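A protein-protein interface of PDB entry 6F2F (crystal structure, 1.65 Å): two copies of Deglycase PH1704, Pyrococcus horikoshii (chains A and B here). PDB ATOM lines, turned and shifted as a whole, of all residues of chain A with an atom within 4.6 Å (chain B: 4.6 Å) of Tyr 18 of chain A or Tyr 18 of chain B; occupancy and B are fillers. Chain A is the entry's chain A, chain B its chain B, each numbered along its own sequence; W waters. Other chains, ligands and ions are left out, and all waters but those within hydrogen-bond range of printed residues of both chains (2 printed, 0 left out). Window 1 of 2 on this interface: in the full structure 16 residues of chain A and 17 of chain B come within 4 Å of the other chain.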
ATOM      1  N   VAL A  14     -24.945  -4.996 -11.494  1.00  0.00           N
ATOM      2  CA  VAL A  14     -24.529  -5.950 -12.526  1.00  0.00           C
ATOM      3  C   VAL A  14     -25.649  -6.873 -12.968  1.00  0.00           C
ATOM      4  O   VAL A  14     -25.654  -7.341 -14.106  1.00  0.00           O
ATOM      5  CB  VAL A  14     -23.269  -6.753 -12.155  1.00  0.00           C
ATOM      6  CG1 VAL A  14     -22.079  -5.834 -11.974  1.00  0.00           C
ATOM      7  CG2 VAL A  14     -23.487  -7.639 -10.922  1.00  0.00           C
ATOM      8  N   LEU A  16     -28.692  -5.980 -13.644  1.00  0.00           N
ATOM      9  CA  LEU A  16     -29.377  -5.252 -14.701  1.00  0.00           C
ATOM     10  C   LEU A  16     -28.441  -5.043 -15.886  1.00  0.00           C
ATOM     11  O   LEU A  16     -28.805  -5.343 -17.028  1.00  0.00           O
ATOM     12  CB  LEU A  16     -29.838  -3.876 -14.192  1.00  0.00           C
ATOM     13  CG  LEU A  16     -30.658  -3.008 -15.163  1.00  0.00           C
ATOM     14  CD1 LEU A  16     -31.424  -1.929 -14.394  1.00  0.00           C
ATOM     15  CD2 LEU A  16     -29.813  -2.309 -16.181  1.00  0.00           C
ATOM     16  N   ILE A  17     -27.226  -4.534 -15.621  1.00  0.00           N
ATOM     17  CA  ILE A  17     -26.311  -4.170 -16.708  1.00  0.00           C
ATOM     18  C   ILE A  17     -25.854  -5.394 -17.530  1.00  0.00           C
ATOM     19  O   ILE A  17     -25.792  -5.303 -18.770  1.00  0.00           O
ATOM     20  CB  ILE A  17     -25.143  -3.328 -16.167  1.00  0.00           C
ATOM     21  CG1 ILE A  17     -25.672  -1.971 -15.615  1.00  0.00           C
ATOM     22  CG2 ILE A  17     -24.055  -3.079 -17.248  1.00  0.00           C
ATOM     23  CD1 ILE A  17     -24.685  -1.259 -14.694  1.00  0.00           C
ATOM     24  N   TYR A  18     -25.544  -6.500 -16.878  1.00  0.00           N
ATOM     25  CA  TYR A  18     -25.111  -7.702 -17.570  1.00  0.00           C
ATOM     26  C   TYR A  18     -26.131  -8.231 -18.573  1.00  0.00           C
ATOM     27  O   TYR A  18     -25.828  -8.287 -19.764  1.00  0.00           O
ATOM     28  CB  TYR A  18     -24.657  -8.785 -16.596  1.00  0.00           C
ATOM     29  CG  TYR A  18     -24.036  -9.956 -17.321  1.00  0.00           C
ATOM     30  CD1 TYR A  18     -22.681  -9.953 -17.669  1.00  0.00           C
ATOM     31  CD2 TYR A  18     -24.798 -11.053 -17.697  1.00  0.00           C
ATOM     32  CE1 TYR A  18     -22.132 -10.974 -18.419  1.00  0.00           C
ATOM     33  CE2 TYR A  18     -24.234 -12.117 -18.395  1.00  0.00           C
ATOM     34  CZ  TYR A  18     -22.897 -12.057 -18.782  1.00  0.00           C
ATOM     35  OH  TYR A  18     -22.293 -13.075 -19.437  1.00  0.00           O
ATOM     36  N   PRO A  19     -27.388  -8.548 -18.182  1.00  0.00           N
ATOM     37  CA  PRO A  19     -28.342  -9.032 -19.190  1.00  0.00           C
ATOM     38  C   PRO A  19     -28.688  -7.966 -20.221  1.00  0.00           C
ATOM     39  O   PRO A  19     -28.962  -8.292 -21.383  1.00  0.00           O
ATOM     40  CB  PRO A  19     -29.570  -9.434 -18.360  1.00  0.00           C
ATOM     41  CG  PRO A  19     -29.431  -8.647 -17.092  1.00  0.00           C
ATOM     42  CD  PRO A  19     -27.946  -8.634 -16.825  1.00  0.00           C
ATOM     43  N   TYR A  20     -28.655  -6.690 -19.838  1.00  0.00           N
ATOM     44  CA  TYR A  20     -28.947  -5.612 -20.790  1.00  0.00           C
ATOM     45  C   TYR A  20     -27.984  -5.696 -21.963  1.00  0.00           C
ATOM     46  O   TYR A  20     -28.406  -5.754 -23.121  1.00  0.00           O
ATOM     47  CB  TYR A  20     -28.816  -4.269 -20.051  1.00  0.00           C
ATOM     48  CG  TYR A  20     -29.229  -3.051 -20.846  1.00  0.00           C
ATOM     49  CD1 TYR A  20     -28.325  -2.393 -21.656  1.00  0.00           C
ATOM     50  CD2 TYR A  20     -30.557  -2.621 -20.861  1.00  0.00           C
ATOM     51  CE1 TYR A  20     -28.703  -1.273 -22.396  1.00  0.00           C
ATOM     52  CE2 TYR A  20     -30.943  -1.488 -21.575  1.00  0.00           C
ATOM     53  CZ  TYR A  20     -30.016  -0.815 -22.342  1.00  0.00           C
ATOM     54  OH  TYR A  20     -30.436   0.277 -23.086  1.00  0.00           O
ATOM     55  N   HIS A  21     -26.685  -5.735 -21.678  1.00  0.00           N
ATOM     56  CA  HIS A  21     -25.704  -5.812 -22.745  1.00  0.00           C
ATOM     57  C   HIS A  21     -25.666  -7.174 -23.418  1.00  0.00           C
ATOM     58  O   HIS A  21     -25.501  -7.261 -24.637  1.00  0.00           O
ATOM     59  CB  HIS A  21     -24.297  -5.418 -22.219  1.00  0.00           C
ATOM     60  CG  HIS A  21     -24.168  -3.941 -22.085  1.00  0.00           C
ATOM     61  ND1 HIS A  21     -23.814  -3.133 -23.169  1.00  0.00           N
ATOM     62  CD2 HIS A  21     -24.474  -3.159 -21.037  1.00  0.00           C
ATOM     63  CE1 HIS A  21     -23.885  -1.895 -22.712  1.00  0.00           C
ATOM     64  NE2 HIS A  21     -24.288  -1.864 -21.434  1.00  0.00           N
ATOM     65  N   ARG A  22     -25.812  -8.243 -22.650  1.00  0.00           N
ATOM     66  CA  ARG A  22     -25.776  -9.578 -23.240  1.00  0.00           C
ATOM     67  C   ARG A  22     -26.866  -9.774 -24.274  1.00  0.00           C
ATOM     68  O   ARG A  22     -26.640 -10.403 -25.325  1.00  0.00           O
ATOM     69  CB  ARG A  22     -25.861 -10.641 -22.151  1.00  0.00           C
ATOM     70  CG  ARG A  22     -25.783 -12.068 -22.695  1.00  0.00           C
ATOM     71  CD  ARG A  22     -24.427 -12.413 -23.301  1.00  0.00           C
ATOM     72  NE  ARG A  22     -24.447 -13.707 -23.993  1.00  0.00           N
ATOM     73  CZ  ARG A  22     -24.773 -13.904 -25.272  1.00  0.00           C
ATOM     74  NH1 ARG A  22     -25.218 -12.895 -26.020  1.00  0.00           N
ATOM     75  NH2 ARG A  22     -24.710 -15.121 -25.800  1.00  0.00           N
ATOM     76  N   GLU A  25     -26.198  -7.763 -27.443  1.00  0.00           N
ATOM     77  CA  GLU A  25     -25.229  -8.447 -28.300  1.00  0.00           C
ATOM     78  C   GLU A  25     -25.936  -9.291 -29.363  1.00  0.00           C
ATOM     79  O   GLU A  25     -25.493  -9.349 -30.513  1.00  0.00           O
ATOM     80  CB  GLU A  25     -24.316  -9.363 -27.468  1.00  0.00           C
ATOM     81  CG  GLU A  25     -23.540 -10.332 -28.333  1.00  0.00           C
ATOM     82  CD  GLU A  25     -22.559 -11.234 -27.620  1.00  0.00           C
ATOM     83  OE1 GLU A  25     -22.149 -12.249 -28.222  1.00  0.00           O
ATOM     84  OE2 GLU A  25     -22.327 -11.022 -26.413  1.00  0.00           O
ATOM     85  N   LEU A 154     -24.136 -15.026 -13.090  1.00  0.00           N
ATOM     86  CA  LEU A 154     -24.490 -14.331 -14.330  1.00  0.00           C
ATOM     87  C   LEU A 154     -24.180 -15.096 -15.590  1.00  0.00           C
ATOM     88  O   LEU A 154     -25.014 -15.143 -16.491  1.00  0.00           O
ATOM     89  CB  LEU A 154     -23.858 -12.942 -14.399  1.00  0.00           C
ATOM     90  CG  LEU A 154     -24.369 -11.890 -13.427  1.00  0.00           C
ATOM     91  CD1 LEU A 154     -23.403 -10.688 -13.398  1.00  0.00           C
ATOM     92  CD2 LEU A 154     -25.771 -11.462 -13.761  1.00  0.00           C
ATOM     93  N   TYR A 155     -22.965 -15.626 -15.706  1.00  0.00           N
ATOM     94  CA  TYR A 155     -22.566 -16.335 -16.933  1.00  0.00           C
ATOM     95  C   TYR A 155     -23.554 -17.426 -17.312  1.00  0.00           C
ATOM     96  O   TYR A 155     -23.946 -17.544 -18.476  1.00  0.00           O
ATOM     97  CB  TYR A 155     -21.139 -16.897 -16.792  1.00  0.00           C
ATOM     98  CG  TYR A 155     -21.007 -18.151 -15.950  1.00  0.00           C
ATOM     99  CD1 TYR A 155     -21.060 -18.097 -14.560  1.00  0.00           C
ATOM    100  CD2 TYR A 155     -20.832 -19.391 -16.545  1.00  0.00           C
ATOM    101  CE1 TYR A 155     -20.977 -19.257 -13.790  1.00  0.00           C
ATOM    102  CE2 TYR A 155     -20.697 -20.543 -15.787  1.00  0.00           C
ATOM    103  CZ  TYR A 155     -20.811 -20.478 -14.417  1.00  0.00           C
ATOM    104  OH  TYR A 155     -20.641 -21.660 -13.740  1.00  0.00           O
ATOM    105  N   MET A 158     -27.528 -16.049 -18.222  1.00  0.00           N
ATOM    106  CA  MET A 158     -27.796 -15.622 -19.597  1.00  0.00           C
ATOM    107  C   MET A 158     -27.402 -16.664 -20.619  1.00  0.00           C
ATOM    108  O   MET A 158     -27.977 -16.671 -21.711  1.00  0.00           O
ATOM    109  CB  MET A 158     -27.176 -14.287 -19.918  1.00  0.00           C
ATOM    110  CG  MET A 158     -27.846 -13.135 -19.234  1.00  0.00           C
ATOM    111  SD  MET A 158     -29.533 -12.858 -19.864  1.00  0.00           S
ATOM    112  CE  MET A 158     -30.546 -13.338 -18.445  1.00  0.00           C
ATOM    113  N   VAL B  14     -18.060  -2.805 -13.971  1.00  0.00           N
ATOM    114  CA  VAL B  14     -18.705  -3.559 -15.043  1.00  0.00           C
ATOM    115  C   VAL B  14     -17.744  -3.911 -16.169  1.00  0.00           C
ATOM    116  O   VAL B  14     -17.940  -4.932 -16.848  1.00  0.00           O
ATOM    117  CB  VAL B  14     -19.976  -2.886 -15.586  1.00  0.00           C
ATOM    118  CG1 VAL B  14     -21.039  -2.787 -14.504  1.00  0.00           C
ATOM    119  CG2 VAL B  14     -19.692  -1.524 -16.224  1.00  0.00           C
ATOM    120  N   LEU B  16     -14.780  -5.078 -15.795  1.00  0.00           N
ATOM    121  CA  LEU B  16     -14.161  -6.330 -15.387  1.00  0.00           C
ATOM    122  C   LEU B  16     -15.223  -7.422 -15.340  1.00  0.00           C
ATOM    123  O   LEU B  16     -15.043  -8.514 -15.912  1.00  0.00           O
ATOM    124  CB  LEU B  16     -13.482  -6.190 -14.009  1.00  0.00           C
ATOM    125  CG  LEU B  16     -12.736  -7.431 -13.464  1.00  0.00           C
ATOM    126  CD1 LEU B  16     -11.848  -7.043 -12.245  1.00  0.00           C
ATOM    127  CD2 LEU B  16     -13.643  -8.494 -12.962  1.00  0.00           C
ATOM    128  N   ILE B  17     -16.336  -7.173 -14.620  1.00  0.00           N
ATOM    129  CA  ILE B  17     -17.340  -8.205 -14.376  1.00  0.00           C
ATOM    130  C   ILE B  17     -18.054  -8.683 -15.651  1.00  0.00           C
ATOM    131  O   ILE B  17     -18.261  -9.904 -15.820  1.00  0.00           O
ATOM    132  CB  ILE B  17     -18.342  -7.728 -13.287  1.00  0.00           C
ATOM    133  CG1 ILE B  17     -17.600  -7.535 -11.944  1.00  0.00           C
ATOM    134  CG2 ILE B  17     -19.510  -8.708 -13.139  1.00  0.00           C
ATOM    135  CD1 ILE B  17     -18.375  -6.687 -10.934  1.00  0.00           C
ATOM    136  N   TYR B  18     -18.348  -7.777 -16.561  1.00  0.00           N
ATOM    137  CA  TYR B  18     -19.017  -8.168 -17.810  1.00  0.00           C
ATOM    138  C   TYR B  18     -18.216  -9.137 -18.657  1.00  0.00           C
ATOM    139  O   TYR B  18     -18.679 -10.252 -18.923  1.00  0.00           O
ATOM    140  CB  TYR B  18     -19.441  -6.919 -18.611  1.00  0.00           C
ATOM    141  CG  TYR B  18     -20.275  -7.305 -19.812  1.00  0.00           C
ATOM    142  CD1 TYR B  18     -21.644  -7.515 -19.691  1.00  0.00           C
ATOM    143  CD2 TYR B  18     -19.690  -7.534 -21.041  1.00  0.00           C
ATOM    144  CE1 TYR B  18     -22.407  -7.956 -20.765  1.00  0.00           C
ATOM    145  CE2 TYR B  18     -20.447  -7.931 -22.140  1.00  0.00           C
ATOM    146  CZ  TYR B  18     -21.810  -8.160 -21.993  1.00  0.00           C
ATOM    147  OH  TYR B  18     -22.603  -8.528 -23.053  1.00  0.00           O
ATOM    148  N   PRO B  19     -16.941  -8.834 -19.043  1.00  0.00           N
ATOM    149  CA  PRO B  19     -16.194  -9.810 -19.828  1.00  0.00           C
ATOM    150  C   PRO B  19     -15.903 -11.081 -19.054  1.00  0.00           C
ATOM    151  O   PRO B  19     -15.824 -12.159 -19.653  1.00  0.00           O
ATOM    152  CB  PRO B  19     -14.919  -9.058 -20.208  1.00  0.00           C
ATOM    153  CG  PRO B  19     -14.796  -7.968 -19.173  1.00  0.00           C
ATOM    154  CD  PRO B  19     -16.219  -7.554 -18.916  1.00  0.00           C
ATOM    155  N   TYR B  20     -15.730 -10.982 -17.731  1.00  0.00           N
ATOM    156  CA  TYR B  20     -15.474 -12.160 -16.920  1.00  0.00           C
ATOM    157  C   TYR B  20     -16.563 -13.176 -17.128  1.00  0.00           C
ATOM    158  O   TYR B  20     -16.307 -14.343 -17.458  1.00  0.00           O
ATOM    159  CB  TYR B  20     -15.364 -11.732 -15.443  1.00  0.00           C
ATOM    160  CG  TYR B  20     -14.957 -12.830 -14.492  1.00  0.00           C
ATOM    161  CD1 TYR B  20     -15.905 -13.627 -13.874  1.00  0.00           C
ATOM    162  CD2 TYR B  20     -13.621 -13.050 -14.186  1.00  0.00           C
ATOM    163  CE1 TYR B  20     -15.534 -14.642 -12.991  1.00  0.00           C
ATOM    164  CE2 TYR B  20     -13.243 -14.043 -13.289  1.00  0.00           C
ATOM    165  CZ  TYR B  20     -14.205 -14.818 -12.674  1.00  0.00           C
ATOM    166  OH  TYR B  20     -13.813 -15.800 -11.794  1.00  0.00           O
ATOM    167  N   HIS B  21     -17.821 -12.749 -16.932  1.00  0.00           N
ATOM    168  CA  HIS B  21     -18.930 -13.659 -17.102  1.00  0.00           C
ATOM    169  C   HIS B  21     -19.199 -14.021 -18.560  1.00  0.00           C
ATOM    170  O   HIS B  21     -19.536 -15.172 -18.866  1.00  0.00           O
ATOM    171  CB  HIS B  21     -20.199 -13.084 -16.430  1.00  0.00           C
ATOM    172  CG  HIS B  21     -20.151 -13.261 -14.956  1.00  0.00           C
ATOM    173  ND1 HIS B  21     -20.534 -14.442 -14.352  1.00  0.00           N
ATOM    174  CD2 HIS B  21     -19.632 -12.434 -14.018  1.00  0.00           C
ATOM    175  CE1 HIS B  21     -20.268 -14.289 -13.061  1.00  0.00           C
ATOM    176  NE2 HIS B  21     -19.715 -13.094 -12.811  1.00  0.00           N
ATOM    177  N   ARG B  22     -19.060 -13.062 -19.461  1.00  0.00           N
ATOM    178  CA  ARG B  22     -19.338 -13.340 -20.864  1.00  0.00           C
ATOM    179  C   ARG B  22     -18.425 -14.429 -21.405  1.00  0.00           C
ATOM    180  O   ARG B  22     -18.858 -15.285 -22.201  1.00  0.00           O
ATOM    181  CB  ARG B  22     -19.204 -12.068 -21.694  1.00  0.00           C
ATOM    182  CG  ARG B  22     -19.505 -12.281 -23.174  1.00  0.00           C
ATOM    183  CD  ARG B  22     -20.948 -12.646 -23.452  1.00  0.00           C
ATOM    184  NE  ARG B  22     -21.184 -13.042 -24.837  1.00  0.00           N
ATOM    185  CZ  ARG B  22     -21.043 -14.274 -25.341  1.00  0.00           C
ATOM    186  NH1 ARG B  22     -20.602 -15.268 -24.581  1.00  0.00           N
ATOM    187  NH2 ARG B  22     -21.333 -14.516 -26.611  1.00  0.00           N
ATOM    188  N   GLU B  25     -19.286 -17.863 -20.010  1.00  0.00           N
ATOM    189  CA  GLU B  25     -20.436 -18.433 -20.732  1.00  0.00           C
ATOM    190  C   GLU B  25     -19.970 -19.365 -21.842  1.00  0.00           C
ATOM    191  O   GLU B  25     -20.555 -20.418 -22.069  1.00  0.00           O
ATOM    192  CB  GLU B  25     -21.309 -17.334 -21.334  1.00  0.00           C
ATOM    193  CG  GLU B  25     -22.305 -17.888 -22.333  1.00  0.00           C
ATOM    194  CD  GLU B  25     -23.273 -16.908 -22.944  1.00  0.00           C
ATOM    195  OE1 GLU B  25     -23.858 -17.249 -24.003  1.00  0.00           O
ATOM    196  OE2 GLU B  25     -23.325 -15.754 -22.462  1.00  0.00           O
ATOM    197  N   LEU B 154     -20.117  -2.157 -23.916  1.00  0.00           N
ATOM    198  CA  LEU B 154     -19.858  -3.539 -23.532  1.00  0.00           C
ATOM    199  C   LEU B 154     -20.415  -4.571 -24.484  1.00  0.00           C
ATOM    200  O   LEU B 154     -19.737  -5.532 -24.811  1.00  0.00           O
ATOM    201  CB  LEU B 154     -20.349  -3.825 -22.120  1.00  0.00           C
ATOM    202  CG  LEU B 154     -19.609  -3.160 -20.966  1.00  0.00           C
ATOM    203  CD1 LEU B 154     -20.415  -3.273 -19.681  1.00  0.00           C
ATOM    204  CD2 LEU B 154     -18.223  -3.724 -20.787  1.00  0.00           C
ATOM    205  N   TYR B 155     -21.700  -4.432 -24.870  1.00  0.00           N
ATOM    206  CA  TYR B 155     -22.325  -5.432 -25.736  1.00  0.00           C
ATOM    207  C   TYR B 155     -21.497  -5.681 -27.010  1.00  0.00           C
ATOM    208  O   TYR B 155     -21.294  -6.834 -27.422  1.00  0.00           O
ATOM    209  CB  TYR B 155     -23.767  -5.039 -26.076  1.00  0.00           C
ATOM    210  CG  TYR B 155     -23.910  -3.942 -27.105  1.00  0.00           C
ATOM    211  CD1 TYR B 155     -23.667  -2.607 -26.778  1.00  0.00           C
ATOM    212  CD2 TYR B 155     -24.300  -4.233 -28.404  1.00  0.00           C
ATOM    213  CE1 TYR B 155     -23.769  -1.601 -27.742  1.00  0.00           C
ATOM    214  CE2 TYR B 155     -24.443  -3.237 -29.355  1.00  0.00           C
ATOM    215  CZ  TYR B 155     -24.187  -1.922 -29.017  1.00  0.00           C
ATOM    216  OH  TYR B 155     -24.380  -0.989 -30.011  1.00  0.00           O
ATOM    217  N   MET B 158     -17.572  -7.290 -26.333  1.00  0.00           N
ATOM    218  CA  MET B 158     -17.459  -8.748 -26.232  1.00  0.00           C
ATOM    219  C   MET B 158     -18.087  -9.457 -27.392  1.00  0.00           C
ATOM    220  O   MET B 158     -17.690 -10.590 -27.682  1.00  0.00           O
ATOM    221  CB  MET B 158     -17.973  -9.266 -24.912  1.00  0.00           C
ATOM    222  CG  MET B 158     -17.101  -8.923 -23.743  1.00  0.00           C
ATOM    223  SD  MET B 158     -15.481  -9.761 -23.820  1.00  0.00           S
ATOM    224  CE  MET B 158     -14.349  -8.410 -24.123  1.00  0.00           C
HETATM  225  O   HOH W   1     -21.312  -8.779 -25.336  1.00  0.00           O
HETATM  226  O   HOH W   2     -23.886 -15.179 -19.928  1.00  0.00           O
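Water W1 lies within hydrogen-bond range of the side-chain hydroxyl (OH) of Tyr 18 of chain B (2.6 Å), the side-chain carboxylate (OE2) of Glu 25 of chain A (2.7 Å) and the backbone carbonyl oxygen (O) of Tyr 155 of chain B (2.9 Å). Water W2 lies within hydrogen-bond range of OE2 of Glu 25 of chain B, OH of Tyr 18 of chain A and O of Tyr 155 of chain A.
Of the 12 printed residues of chain B, 8 touch a printed residue of chain A. Printed residues of chain B that touch a printed residue of chain A: Val 14, Ile 17, Tyr 18, His 21, Arg 22, Glu 25, Leu 154 and Tyr 155. Hydrophobic or aromatic side chains of chain B that line the printed part of chain A: Val 14, Ile 17, Tyr 18, His 21, Leu 154 and Tyr 155. Hydrophobic or aromatic side chains of chain A within 4 Å of the printed part of chain B: Val 14, Ile 17, Tyr 18, His 21, Leu 154 and Tyr 155. Among the printed residues, 16 pairs touch across the chains.
Of chain B, only Tyr 18, His 21 and Arg 22 come within 4 Å of Tyr 18 of chain A. Of the printed residues of chain A, Val 14 of chain B touches Ile 17 (3.96 Å). Tyr 18 of chain B touches just these residues of chain A: Tyr 18 (3.3 Å), His 21 (3.4 Å) and Arg 22 (3.2 Å). Tyr 20 of chain B touches none of the printed residues of chain A. Printed residues of chain A within 4 Å of Arg 22 of chain B: Tyr 18 (3.2 Å), Arg 22 (3.4 Å) and Glu 25 (2.8 Å). The nearest residue of chain A that does not touch Tyr 18 of chain B is Glu 25 of chain A (4.2 Å). The nearest printed residue of chain A that does not touch Glu 25 of chain B is Tyr 18 of chain A (4.2 Å).
The backbone NH (N) of Arg 22 of chain B is in hydrogen-bond range of the side-chain hydroxyl (OH) of Tyr 18 of chain A. A ring nitrogen (ND1) of His 21 of chain A lies within hydrogen-bond range of the backbone NH of Tyr 155 of chain B, 3.0 Å away. The side-chain hydroxyl of Tyr 18 of chain B sits at hydrogen-bond distance from the backbone NH of Arg 22 of chain A. The side-chain carboxylate (OE2) of Glu 25 of chain B is in salt-bridge range of the guanidinium group (NE) of Arg 22 of chain A, 2.8 Å away. OE2 of Glu 25 of chain A is in salt-bridge range of NE of Arg 22 of chain B, at 2.8 Å. ND1 of His 21 of chain B lies within hydrogen-bond range of N of Tyr 155 of chain A, 3.0 Å away. The guanidinium group (NE) of Arg 22 of chain A sits close to the guanidinium group (NE) of Arg 22 of chain B, at 3.4 Å.
Tyr 18 of chain B touches its own counterpart, Tyr 18 of chain A. His 21 of chain A touches Leu 154 of chain B, and with the chains exchanged Leu 154 of chain A touches His 21 of chain B. Arg 22 of chain A touches its own counterpart, Arg 22 of chain B. Arg 22 of chain A touches Glu 25 of chain B, and with the chains exchanged Glu 25 of chain A touches Arg 22 of chain B. Positions printed for both chains: 14, 16, 17, 18, 19, 20, 21, 22, 25, 154, 155 and 158.
The side-chain carboxylate (OE2) of Glu 25 of chain A is in salt-bridge range of the guanidinium group (NH1) of Arg 22 of chain A (3.5 Å). The side-chain carboxylate of Glu 25 of chain B lies within salt-bridge range of the guanidinium group of Arg 22 of chain B (3.5 Å).
Among the printed residues, pairs that only touch across the chains: Tyr 18 of chain A with Tyr 18 of chain B (3.3 Å), Tyr 18 of chain A with His 21 of chain B (3.4 Å), His 21 of chain A with Tyr 18 of chain B (3.4 Å), Leu 154 of chain A with His 21 of chain B (3.6 Å), His 21 of chain A with Leu 154 of chain B (3.7 Å), Tyr 155 of chain A with Glu 25 of chain B (3.8 Å), Glu 25 of chain A with Tyr 155 of chain B (3.9 Å), Val 14 of chain A with Ile 17 of chain B (3.9 Å) and Ile 17 of chain A with Val 14 of chain B (3.96 Å).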
